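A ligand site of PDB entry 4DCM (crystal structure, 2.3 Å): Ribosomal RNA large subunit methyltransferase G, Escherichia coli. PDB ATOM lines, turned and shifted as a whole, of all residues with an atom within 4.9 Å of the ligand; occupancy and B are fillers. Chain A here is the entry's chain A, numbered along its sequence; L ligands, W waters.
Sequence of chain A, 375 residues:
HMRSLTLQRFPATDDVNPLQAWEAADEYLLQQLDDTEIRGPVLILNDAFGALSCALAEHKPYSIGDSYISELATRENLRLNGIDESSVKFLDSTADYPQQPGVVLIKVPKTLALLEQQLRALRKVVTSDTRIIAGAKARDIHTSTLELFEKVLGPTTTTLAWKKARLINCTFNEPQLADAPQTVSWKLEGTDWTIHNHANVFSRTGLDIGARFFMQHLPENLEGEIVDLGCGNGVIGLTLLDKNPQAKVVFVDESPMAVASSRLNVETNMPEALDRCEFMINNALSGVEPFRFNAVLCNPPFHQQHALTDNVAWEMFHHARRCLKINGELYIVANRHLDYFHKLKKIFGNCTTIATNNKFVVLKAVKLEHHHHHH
O of Gly 232 sits close to O of Ala 258 (2.7 Å). OD1 of Asp 253 is in hydrogen-bond range of N of Gly 232, at 3.0 Å. OD2 of Asp 253 lies within hydrogen-bond range of N of Ser 255, at 2.9 Å. N of Asn 282 is in hydrogen-bond range of O of Asp 253, at 3.1 Å. The side-chain carboxylate (OD1) of Asp 253 lies within hydrogen-bond range of the backbone NH (N) of Cys 231 (3.4 Å). N of Gly 230 lies within hydrogen-bond range of O of Val 252. The backbone carbonyl oxygen (O) of Ala 284 is in hydrogen-bond range of the side-chain amide nitrogen (ND2) of Asn 282, at 3.3 Å. The backbone NH (N) of Cys 231 is in hydrogen-bond range of the backbone carbonyl oxygen (O) of Val 252, 2.9 Å away.
CD2 of Phe 202 touches S1 of the ligand, at 3.5 Å. CB of Ala 211 touches O1 of the ligand, at 3.3 Å. Gly 232 touches the ligand. Ile 236 touches the ligand (CG1 to O2, 3.6 Å). O of Asn 282 touches C14 of the ligand, 3.5 Å away. O of Pro 300 touches C5 of the ligand, at 3.8 Å. Pro 301 touches the ligand. Met 316 touches the ligand. Hydrophobic or aromatic side chains that line the ligand: Phe 202, Ala 211, Ile 236, Pro 301 and Met 316. Of the 24 residues printed, 16 come within 4 Å of the ligand. The nearest printed residue that does not touch the ligand is Val 312 (4.1 Å).
N of Glu 254 sits at hydrogen-bond distance from N6 of the ligand, at 3.2 Å. A nitrogen (N4) of the ligand sits at hydrogen-bond distance from the side-chain amide oxygen (OD1) of Asn 283, at 3.2 Å. An oxygen (O2) of the ligand sits at hydrogen-bond distance from the side-chain amide nitrogen (ND2) of Asn 299 (3.0 Å). The side-chain carboxylate of Asp 253 sits at hydrogen-bond distance from an oxygen (O5) of the ligand (2.8 Å). The backbone NH of Ala 284 lies within hydrogen-bond range of a nitrogen (N5) of the ligand. A nitrogen (N1) of the ligand is in hydrogen-bond range of the backbone carbonyl oxygen (O) of Cys 231 (3.2 Å). OD1 of Asp 228 is in salt-bridge range of N1 of the ligand (3.9 Å). O of Gly 230 sits at hydrogen-bond distance from N1 of the ligand, 2.8 Å away.
Water W2 bridges an oxygen (O4) of the ligand (2.6 Å) and the backbone NH of Phe 202 (3.0 Å). Water W1 lies within hydrogen-bond range of O of Cys 231 (2.6 Å), OD2 of Asp 228 (2.9 Å), N of Ile 236 (3.0 Å) and N1 of the ligand (3.0 Å).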
ATOM      1  N   ILE A  69      12.670 -15.639   0.109  1.00  0.00           N
ATOM      2  CA  ILE A  69      12.860 -16.550   1.235  1.00  0.00           C
ATOM      3  C   ILE A  69      11.582 -17.367   1.421  1.00  0.00           C
ATOM      4  O   ILE A  69      11.629 -18.558   1.719  1.00  0.00           O
ATOM      5  CB  ILE A  69      13.158 -15.806   2.542  1.00  0.00           C
ATOM      6  CG1 ILE A  69      14.547 -15.167   2.482  1.00  0.00           C
ATOM      7  CG2 ILE A  69      13.084 -16.766   3.724  1.00  0.00           C
ATOM      8  CD1 ILE A  69      15.659 -16.055   3.009  1.00  0.00           C
ATOM      9  N   PHE A 202      12.488  -0.931   1.867  1.00  0.00           N
ATOM     10  CA  PHE A 202      12.991  -0.332   3.104  1.00  0.00           C
ATOM     11  C   PHE A 202      13.158   1.185   2.978  1.00  0.00           C
ATOM     12  O   PHE A 202      13.693   1.684   1.987  1.00  0.00           O
ATOM     13  CB  PHE A 202      14.347  -0.959   3.439  1.00  0.00           C
ATOM     14  CG  PHE A 202      15.115  -0.223   4.511  1.00  0.00           C
ATOM     15  CD1 PHE A 202      14.785  -0.369   5.849  1.00  0.00           C
ATOM     16  CD2 PHE A 202      16.179   0.604   4.171  1.00  0.00           C
ATOM     17  CE1 PHE A 202      15.496   0.301   6.844  1.00  0.00           C
ATOM     18  CE2 PHE A 202      16.903   1.278   5.160  1.00  0.00           C
ATOM     19  CZ  PHE A 202      16.563   1.133   6.494  1.00  0.00           C
ATOM     20  N   ASP A 208      17.345   6.885   4.059  1.00  0.00           N
ATOM     21  CA  ASP A 208      17.708   6.350   5.366  1.00  0.00           C
ATOM     22  C   ASP A 208      18.994   7.005   5.854  1.00  0.00           C
ATOM     23  O   ASP A 208      19.943   7.180   5.083  1.00  0.00           O
ATOM     24  CB  ASP A 208      17.879   4.837   5.286  1.00  0.00           C
ATOM     25  CG  ASP A 208      18.409   4.241   6.576  1.00  0.00           C
ATOM     26  OD1 ASP A 208      17.647   4.179   7.566  1.00  0.00           O
ATOM     27  OD2 ASP A 208      19.588   3.816   6.597  1.00  0.00           O
ATOM     28  N   ALA A 211      22.079   4.844   5.682  1.00  0.00           N
ATOM     29  CA  ALA A 211      22.595   4.877   4.319  1.00  0.00           C
ATOM     30  C   ALA A 211      23.299   6.203   4.019  1.00  0.00           C
ATOM     31  O   ALA A 211      24.354   6.221   3.395  1.00  0.00           O
ATOM     32  CB  ALA A 211      21.460   4.640   3.309  1.00  0.00           C
ATOM     33  N   ASP A 228      26.134  -4.721  -3.793  1.00  0.00           N
ATOM     34  CA  ASP A 228      25.193  -4.031  -2.923  1.00  0.00           C
ATOM     35  C   ASP A 228      24.315  -5.119  -2.282  1.00  0.00           C
ATOM     36  O   ASP A 228      23.245  -5.481  -2.826  1.00  0.00           O
ATOM     37  CB  ASP A 228      24.342  -3.045  -3.718  1.00  0.00           C
ATOM     38  CG  ASP A 228      23.525  -2.133  -2.833  1.00  0.00           C
ATOM     39  OD1 ASP A 228      23.457  -2.394  -1.601  1.00  0.00           O
ATOM     40  OD2 ASP A 228      22.939  -1.154  -3.361  1.00  0.00           O
ATOM     41  N   LEU A 229      24.774  -5.652  -1.151  1.00  0.00           N
ATOM     42  CA  LEU A 229      24.118  -6.808  -0.536  1.00  0.00           C
ATOM     43  C   LEU A 229      22.974  -6.339   0.337  1.00  0.00           C
ATOM     44  O   LEU A 229      23.201  -5.737   1.382  1.00  0.00           O
ATOM     45  CB  LEU A 229      25.113  -7.625   0.292  1.00  0.00           C
ATOM     46  CG  LEU A 229      24.516  -8.855   0.997  1.00  0.00           C
ATOM     47  CD1 LEU A 229      23.688  -9.716   0.040  1.00  0.00           C
ATOM     48  CD2 LEU A 229      25.621  -9.685   1.634  1.00  0.00           C
ATOM     49  N   GLY A 230      21.749  -6.633  -0.087  1.00  0.00           N
ATOM     50  CA  GLY A 230      20.559  -6.076   0.556  1.00  0.00           C
ATOM     51  C   GLY A 230      20.347  -4.659   0.054  1.00  0.00           C
ATOM     52  O   GLY A 230      20.377  -3.701   0.832  1.00  0.00           O
ATOM     53  N   CYS A 231      20.131  -4.539  -1.258  1.00  0.00           N
ATOM     54  CA  CYS A 231      20.181  -3.245  -1.939  1.00  0.00           C
ATOM     55  C   CYS A 231      18.982  -2.323  -1.656  1.00  0.00           C
ATOM     56  O   CYS A 231      19.128  -1.101  -1.680  1.00  0.00           O
ATOM     57  CB  CYS A 231      20.328  -3.456  -3.452  1.00  0.00           C
ATOM     58  SG  CYS A 231      19.095  -4.581  -4.205  1.00  0.00           S
ATOM     59  N   GLY A 232      17.810  -2.896  -1.390  1.00  0.00           N
ATOM     60  CA  GLY A 232      16.620  -2.081  -1.206  1.00  0.00           C
ATOM     61  C   GLY A 232      16.363  -1.221  -2.441  1.00  0.00           C
ATOM     62  O   GLY A 232      16.249  -1.753  -3.551  1.00  0.00           O
ATOM     63  N   ILE A 236      22.833   2.836  -2.441  1.00  0.00           N
ATOM     64  CA  ILE A 236      24.241   2.512  -2.240  1.00  0.00           C
ATOM     65  C   ILE A 236      24.847   2.036  -3.557  1.00  0.00           C
ATOM     66  O   ILE A 236      25.943   2.470  -3.932  1.00  0.00           O
ATOM     67  CB  ILE A 236      24.445   1.425  -1.186  1.00  0.00           C
ATOM     68  CG1 ILE A 236      23.983   1.935   0.189  1.00  0.00           C
ATOM     69  CG2 ILE A 236      25.918   1.006  -1.127  1.00  0.00           C
ATOM     70  CD1 ILE A 236      24.657   3.224   0.624  1.00  0.00           C
ATOM     71  N   VAL A 252      21.744  -6.970  -4.884  1.00  0.00           N
ATOM     72  CA  VAL A 252      21.189  -8.211  -4.358  1.00  0.00           C
ATOM     73  C   VAL A 252      20.139  -7.962  -3.279  1.00  0.00           C
ATOM     74  O   VAL A 252      20.413  -7.274  -2.292  1.00  0.00           O
ATOM     75  CB  VAL A 252      22.307  -9.096  -3.744  1.00  0.00           C
ATOM     76  CG1 VAL A 252      21.709 -10.378  -3.160  1.00  0.00           C
ATOM     77  CG2 VAL A 252      23.360  -9.418  -4.788  1.00  0.00           C
ATOM     78  N   ASP A 253      18.938  -8.508  -3.458  1.00  0.00           N
ATOM     79  CA  ASP A 253      17.945  -8.430  -2.387  1.00  0.00           C
ATOM     80  C   ASP A 253      16.981  -9.610  -2.389  1.00  0.00           C
ATOM     81  O   ASP A 253      16.733 -10.223  -3.435  1.00  0.00           O
ATOM     82  CB  ASP A 253      17.196  -7.078  -2.396  1.00  0.00           C
ATOM     83  CG  ASP A 253      16.648  -6.703  -1.027  1.00  0.00           C
ATOM     84  OD1 ASP A 253      17.072  -5.661  -0.477  1.00  0.00           O
ATOM     85  OD2 ASP A 253      15.801  -7.465  -0.481  1.00  0.00           O
ATOM     86  N   GLU A 254      16.481  -9.921  -1.207  1.00  0.00           N
ATOM     87  CA  GLU A 254      15.534 -11.023  -0.999  1.00  0.00           C
ATOM     88  C   GLU A 254      14.158 -10.630  -1.519  1.00  0.00           C
ATOM     89  O   GLU A 254      13.318 -11.476  -1.848  1.00  0.00           O
ATOM     90  CB  GLU A 254      15.483 -11.316   0.505  1.00  0.00           C
ATOM     91  CG  GLU A 254      14.639 -12.486   0.905  1.00  0.00           C
ATOM     92  CD  GLU A 254      13.267 -12.066   1.377  1.00  0.00           C
ATOM     93  OE1 GLU A 254      13.134 -10.959   1.948  1.00  0.00           O
ATOM     94  OE2 GLU A 254      12.310 -12.848   1.179  1.00  0.00           O
ATOM     95  N   SER A 255      13.943  -9.318  -1.603  1.00  0.00           N
ATOM     96  CA  SER A 255      12.679  -8.739  -2.013  1.00  0.00           C
ATOM     97  C   SER A 255      12.720  -8.320  -3.480  1.00  0.00           C
ATOM     98  O   SER A 255      13.465  -7.415  -3.850  1.00  0.00           O
ATOM     99  CB  SER A 255      12.414  -7.483  -1.166  1.00  0.00           C
ATOM    100  OG  SER A 255      11.478  -6.616  -1.794  1.00  0.00           O
ATOM    101  N   ALA A 258      12.431  -4.656  -4.026  1.00  0.00           N
ATOM    102  CA  ALA A 258      13.682  -3.931  -3.845  1.00  0.00           C
ATOM    103  C   ALA A 258      14.530  -3.991  -5.124  1.00  0.00           C
ATOM    104  O   ALA A 258      15.033  -2.979  -5.597  1.00  0.00           O
ATOM    105  CB  ALA A 258      14.452  -4.482  -2.671  1.00  0.00           C
ATOM    106  N   ASN A 282      17.923 -12.951  -4.445  1.00  0.00           N
ATOM    107  CA  ASN A 282      18.540 -14.087  -3.797  1.00  0.00           C
ATOM    108  C   ASN A 282      18.462 -14.018  -2.284  1.00  0.00           C
ATOM    109  O   ASN A 282      18.186 -12.963  -1.709  1.00  0.00           O
ATOM    110  CB  ASN A 282      20.012 -14.221  -4.254  1.00  0.00           C
ATOM    111  CG  ASN A 282      20.601 -15.592  -3.971  1.00  0.00           C
ATOM    112  OD1 ASN A 282      19.898 -16.515  -3.537  1.00  0.00           O
ATOM    113  ND2 ASN A 282      21.900 -15.729  -4.208  1.00  0.00           N
ATOM    114  N   ASN A 283      18.681 -15.158  -1.641  1.00  0.00           N
ATOM    115  CA  ASN A 283      18.880 -15.193  -0.210  1.00  0.00           C
ATOM    116  C   ASN A 283      20.358 -14.922   0.035  1.00  0.00           C
ATOM    117  O   ASN A 283      21.194 -15.828  -0.087  1.00  0.00           O
ATOM    118  CB  ASN A 283      18.473 -16.552   0.345  1.00  0.00           C
ATOM    119  CG  ASN A 283      18.955 -16.763   1.754  1.00  0.00           C
ATOM    120  OD1 ASN A 283      19.140 -15.807   2.504  1.00  0.00           O
ATOM    121  ND2 ASN A 283      19.159 -18.029   2.128  1.00  0.00           N
ATOM    122  N   ALA A 284      20.690 -13.679   0.371  1.00  0.00           N
ATOM    123  CA  ALA A 284      22.088 -13.273   0.443  1.00  0.00           C
ATOM    124  C   ALA A 284      22.803 -13.729  -0.813  1.00  0.00           C
ATOM    125  O   ALA A 284      22.417 -13.365  -1.933  1.00  0.00           O
ATOM    126  CB  ALA A 284      22.750 -13.850   1.684  1.00  0.00           C
ATOM    127  N   ASN A 299      24.061  -3.077   4.426  1.00  0.00           N
ATOM    128  CA  ASN A 299      23.371  -2.378   5.508  1.00  0.00           C
ATOM    129  C   ASN A 299      22.314  -3.321   6.063  1.00  0.00           C
ATOM    130  O   ASN A 299      21.127  -3.184   5.764  1.00  0.00           O
ATOM    131  CB  ASN A 299      22.743  -1.081   4.985  1.00  0.00           C
ATOM    132  CG  ASN A 299      22.037  -0.291   6.083  1.00  0.00           C
ATOM    133  OD1 ASN A 299      22.050  -0.680   7.245  1.00  0.00           O
ATOM    134  ND2 ASN A 299      21.409   0.816   5.699  1.00  0.00           N
ATOM    135  N   PRO A 300      22.746  -4.288   6.894  1.00  0.00           N
ATOM    136  CA  PRO A 300      21.931  -5.417   7.349  1.00  0.00           C
ATOM    137  C   PRO A 300      20.654  -4.973   8.032  1.00  0.00           C
ATOM    138  O   PRO A 300      20.611  -3.874   8.584  1.00  0.00           O
ATOM    139  CB  PRO A 300      22.839  -6.128   8.363  1.00  0.00           C
ATOM    140  CG  PRO A 300      24.215  -5.674   8.040  1.00  0.00           C
ATOM    141  CD  PRO A 300      24.079  -4.278   7.520  1.00  0.00           C
ATOM    142  N   PRO A 301      19.617  -5.830   8.002  1.00  0.00           N
ATOM    143  CA  PRO A 301      18.359  -5.473   8.660  1.00  0.00           C
ATOM    144  C   PRO A 301      18.603  -5.229  10.142  1.00  0.00           C
ATOM    145  O   PRO A 301      19.436  -5.888  10.768  1.00  0.00           O
ATOM    146  CB  PRO A 301      17.491  -6.718   8.460  1.00  0.00           C
ATOM    147  CG  PRO A 301      18.063  -7.380   7.225  1.00  0.00           C
ATOM    148  CD  PRO A 301      19.549  -7.140   7.327  1.00  0.00           C
ATOM    149  N   VAL A 312      20.516 -13.134  10.693  1.00  0.00           N
ATOM    150  CA  VAL A 312      20.472 -12.645   9.324  1.00  0.00           C
ATOM    151  C   VAL A 312      21.773 -11.949   8.955  1.00  0.00           C
ATOM    152  O   VAL A 312      22.389 -12.258   7.937  1.00  0.00           O
ATOM    153  CB  VAL A 312      19.308 -11.630   9.148  1.00  0.00           C
ATOM    154  CG1 VAL A 312      19.305 -11.054   7.743  1.00  0.00           C
ATOM    155  CG2 VAL A 312      17.972 -12.286   9.477  1.00  0.00           C
ATOM    156  N   GLU A 315      24.548 -14.366   8.778  1.00  0.00           N
ATOM    157  CA  GLU A 315      24.453 -15.118   7.528  1.00  0.00           C
ATOM    158  C   GLU A 315      25.045 -14.282   6.398  1.00  0.00           C
ATOM    159  O   GLU A 315      25.840 -14.766   5.592  1.00  0.00           O
ATOM    160  CB  GLU A 315      22.985 -15.461   7.227  1.00  0.00           C
ATOM    161  CG  GLU A 315      22.785 -16.765   6.437  1.00  0.00           C
ATOM    162  CD  GLU A 315      21.572 -16.721   5.505  1.00  0.00           C
ATOM    163  OE1 GLU A 315      21.555 -15.880   4.582  1.00  0.00           O
ATOM    164  OE2 GLU A 315      20.639 -17.528   5.703  1.00  0.00           O
ATOM    165  N   MET A 316      24.676 -13.008   6.356  1.00  0.00           N
ATOM    166  CA  MET A 316      25.211 -12.114   5.330  1.00  0.00           C
ATOM    167  C   MET A 316      26.724 -11.990   5.443  1.00  0.00           C
ATOM    168  O   MET A 316      27.428 -12.075   4.452  1.00  0.00           O
ATOM    169  CB  MET A 316      24.527 -10.747   5.387  1.00  0.00           C
ATOM    170  CG  MET A 316      23.132 -10.719   4.770  1.00  0.00           C
ATOM    171  SD  MET A 316      22.232  -8.987   5.040  1.00  0.00           S
ATOM    172  CE  MET A 316      21.067  -9.051   3.471  1.00  0.00           C
HETATM  173  N1  LIG L   1      20.948  -0.992   0.995  1.00  0.00           N
HETATM  174  C1  LIG L   1      19.886  -0.127   1.498  1.00  0.00           C
HETATM  175  C2  LIG L   1      20.467   0.972   2.380  1.00  0.00           C
HETATM  176  O1  LIG L   1      19.760   1.906   2.774  1.00  0.00           O
HETATM  177  O2  LIG L   1      21.661   0.960   2.697  1.00  0.00           O
HETATM  178  C3  LIG L   1      18.823  -0.906   2.263  1.00  0.00           C
HETATM  179  C4  LIG L   1      19.300  -1.658   3.502  1.00  0.00           C
HETATM  180  S1  LIG L   1      17.919  -2.416   4.422  1.00  0.00           S
HETATM  181  C5  LIG L   1      18.382  -2.017   6.132  1.00  0.00           C
HETATM  182  C6  LIG L   1      18.308  -4.186   4.432  1.00  0.00           C
HETATM  183  C7  LIG L   1      17.838  -4.918   3.176  1.00  0.00           C
HETATM  184  O3  LIG L   1      18.224  -6.283   3.200  1.00  0.00           O
HETATM  185  C8  LIG L   1      16.323  -4.907   3.013  1.00  0.00           C
HETATM  186  O4  LIG L   1      16.054  -4.288   1.770  1.00  0.00           O
HETATM  187  C9  LIG L   1      15.915  -6.371   2.985  1.00  0.00           C
HETATM  188  O5  LIG L   1      14.893  -6.647   2.042  1.00  0.00           O
HETATM  189  C10 LIG L   1      17.216  -7.055   2.589  1.00  0.00           C
HETATM  190  N2  LIG L   1      17.328  -8.421   3.092  1.00  0.00           N
HETATM  191  C11 LIG L   1      16.867  -8.907   4.293  1.00  0.00           C
HETATM  192  N3  LIG L   1      17.199 -10.214   4.375  1.00  0.00           N
HETATM  193  C12 LIG L   1      17.862 -10.572   3.255  1.00  0.00           C
HETATM  194  C13 LIG L   1      18.412 -11.786   2.827  1.00  0.00           C
HETATM  195  N4  LIG L   1      18.337 -12.876   3.591  1.00  0.00           N
HETATM  196  N5  LIG L   1      19.045 -11.848   1.600  1.00  0.00           N
HETATM  197  C14 LIG L   1      19.122 -10.721   0.808  1.00  0.00           C
HETATM  198  N6  LIG L   1      18.572  -9.516   1.232  1.00  0.00           N
HETATM  199  C15 LIG L   1      17.958  -9.452   2.432  1.00  0.00           C
HETATM  200  O   HOH W   1      21.218   0.476  -1.614  1.00  0.00           O
HETATM  201  O   HOH W   2      13.965  -3.289   0.629  1.00  0.00           O
HETATM  202  O   HOH W   3      18.011   3.134   1.425  1.00  0.00           O
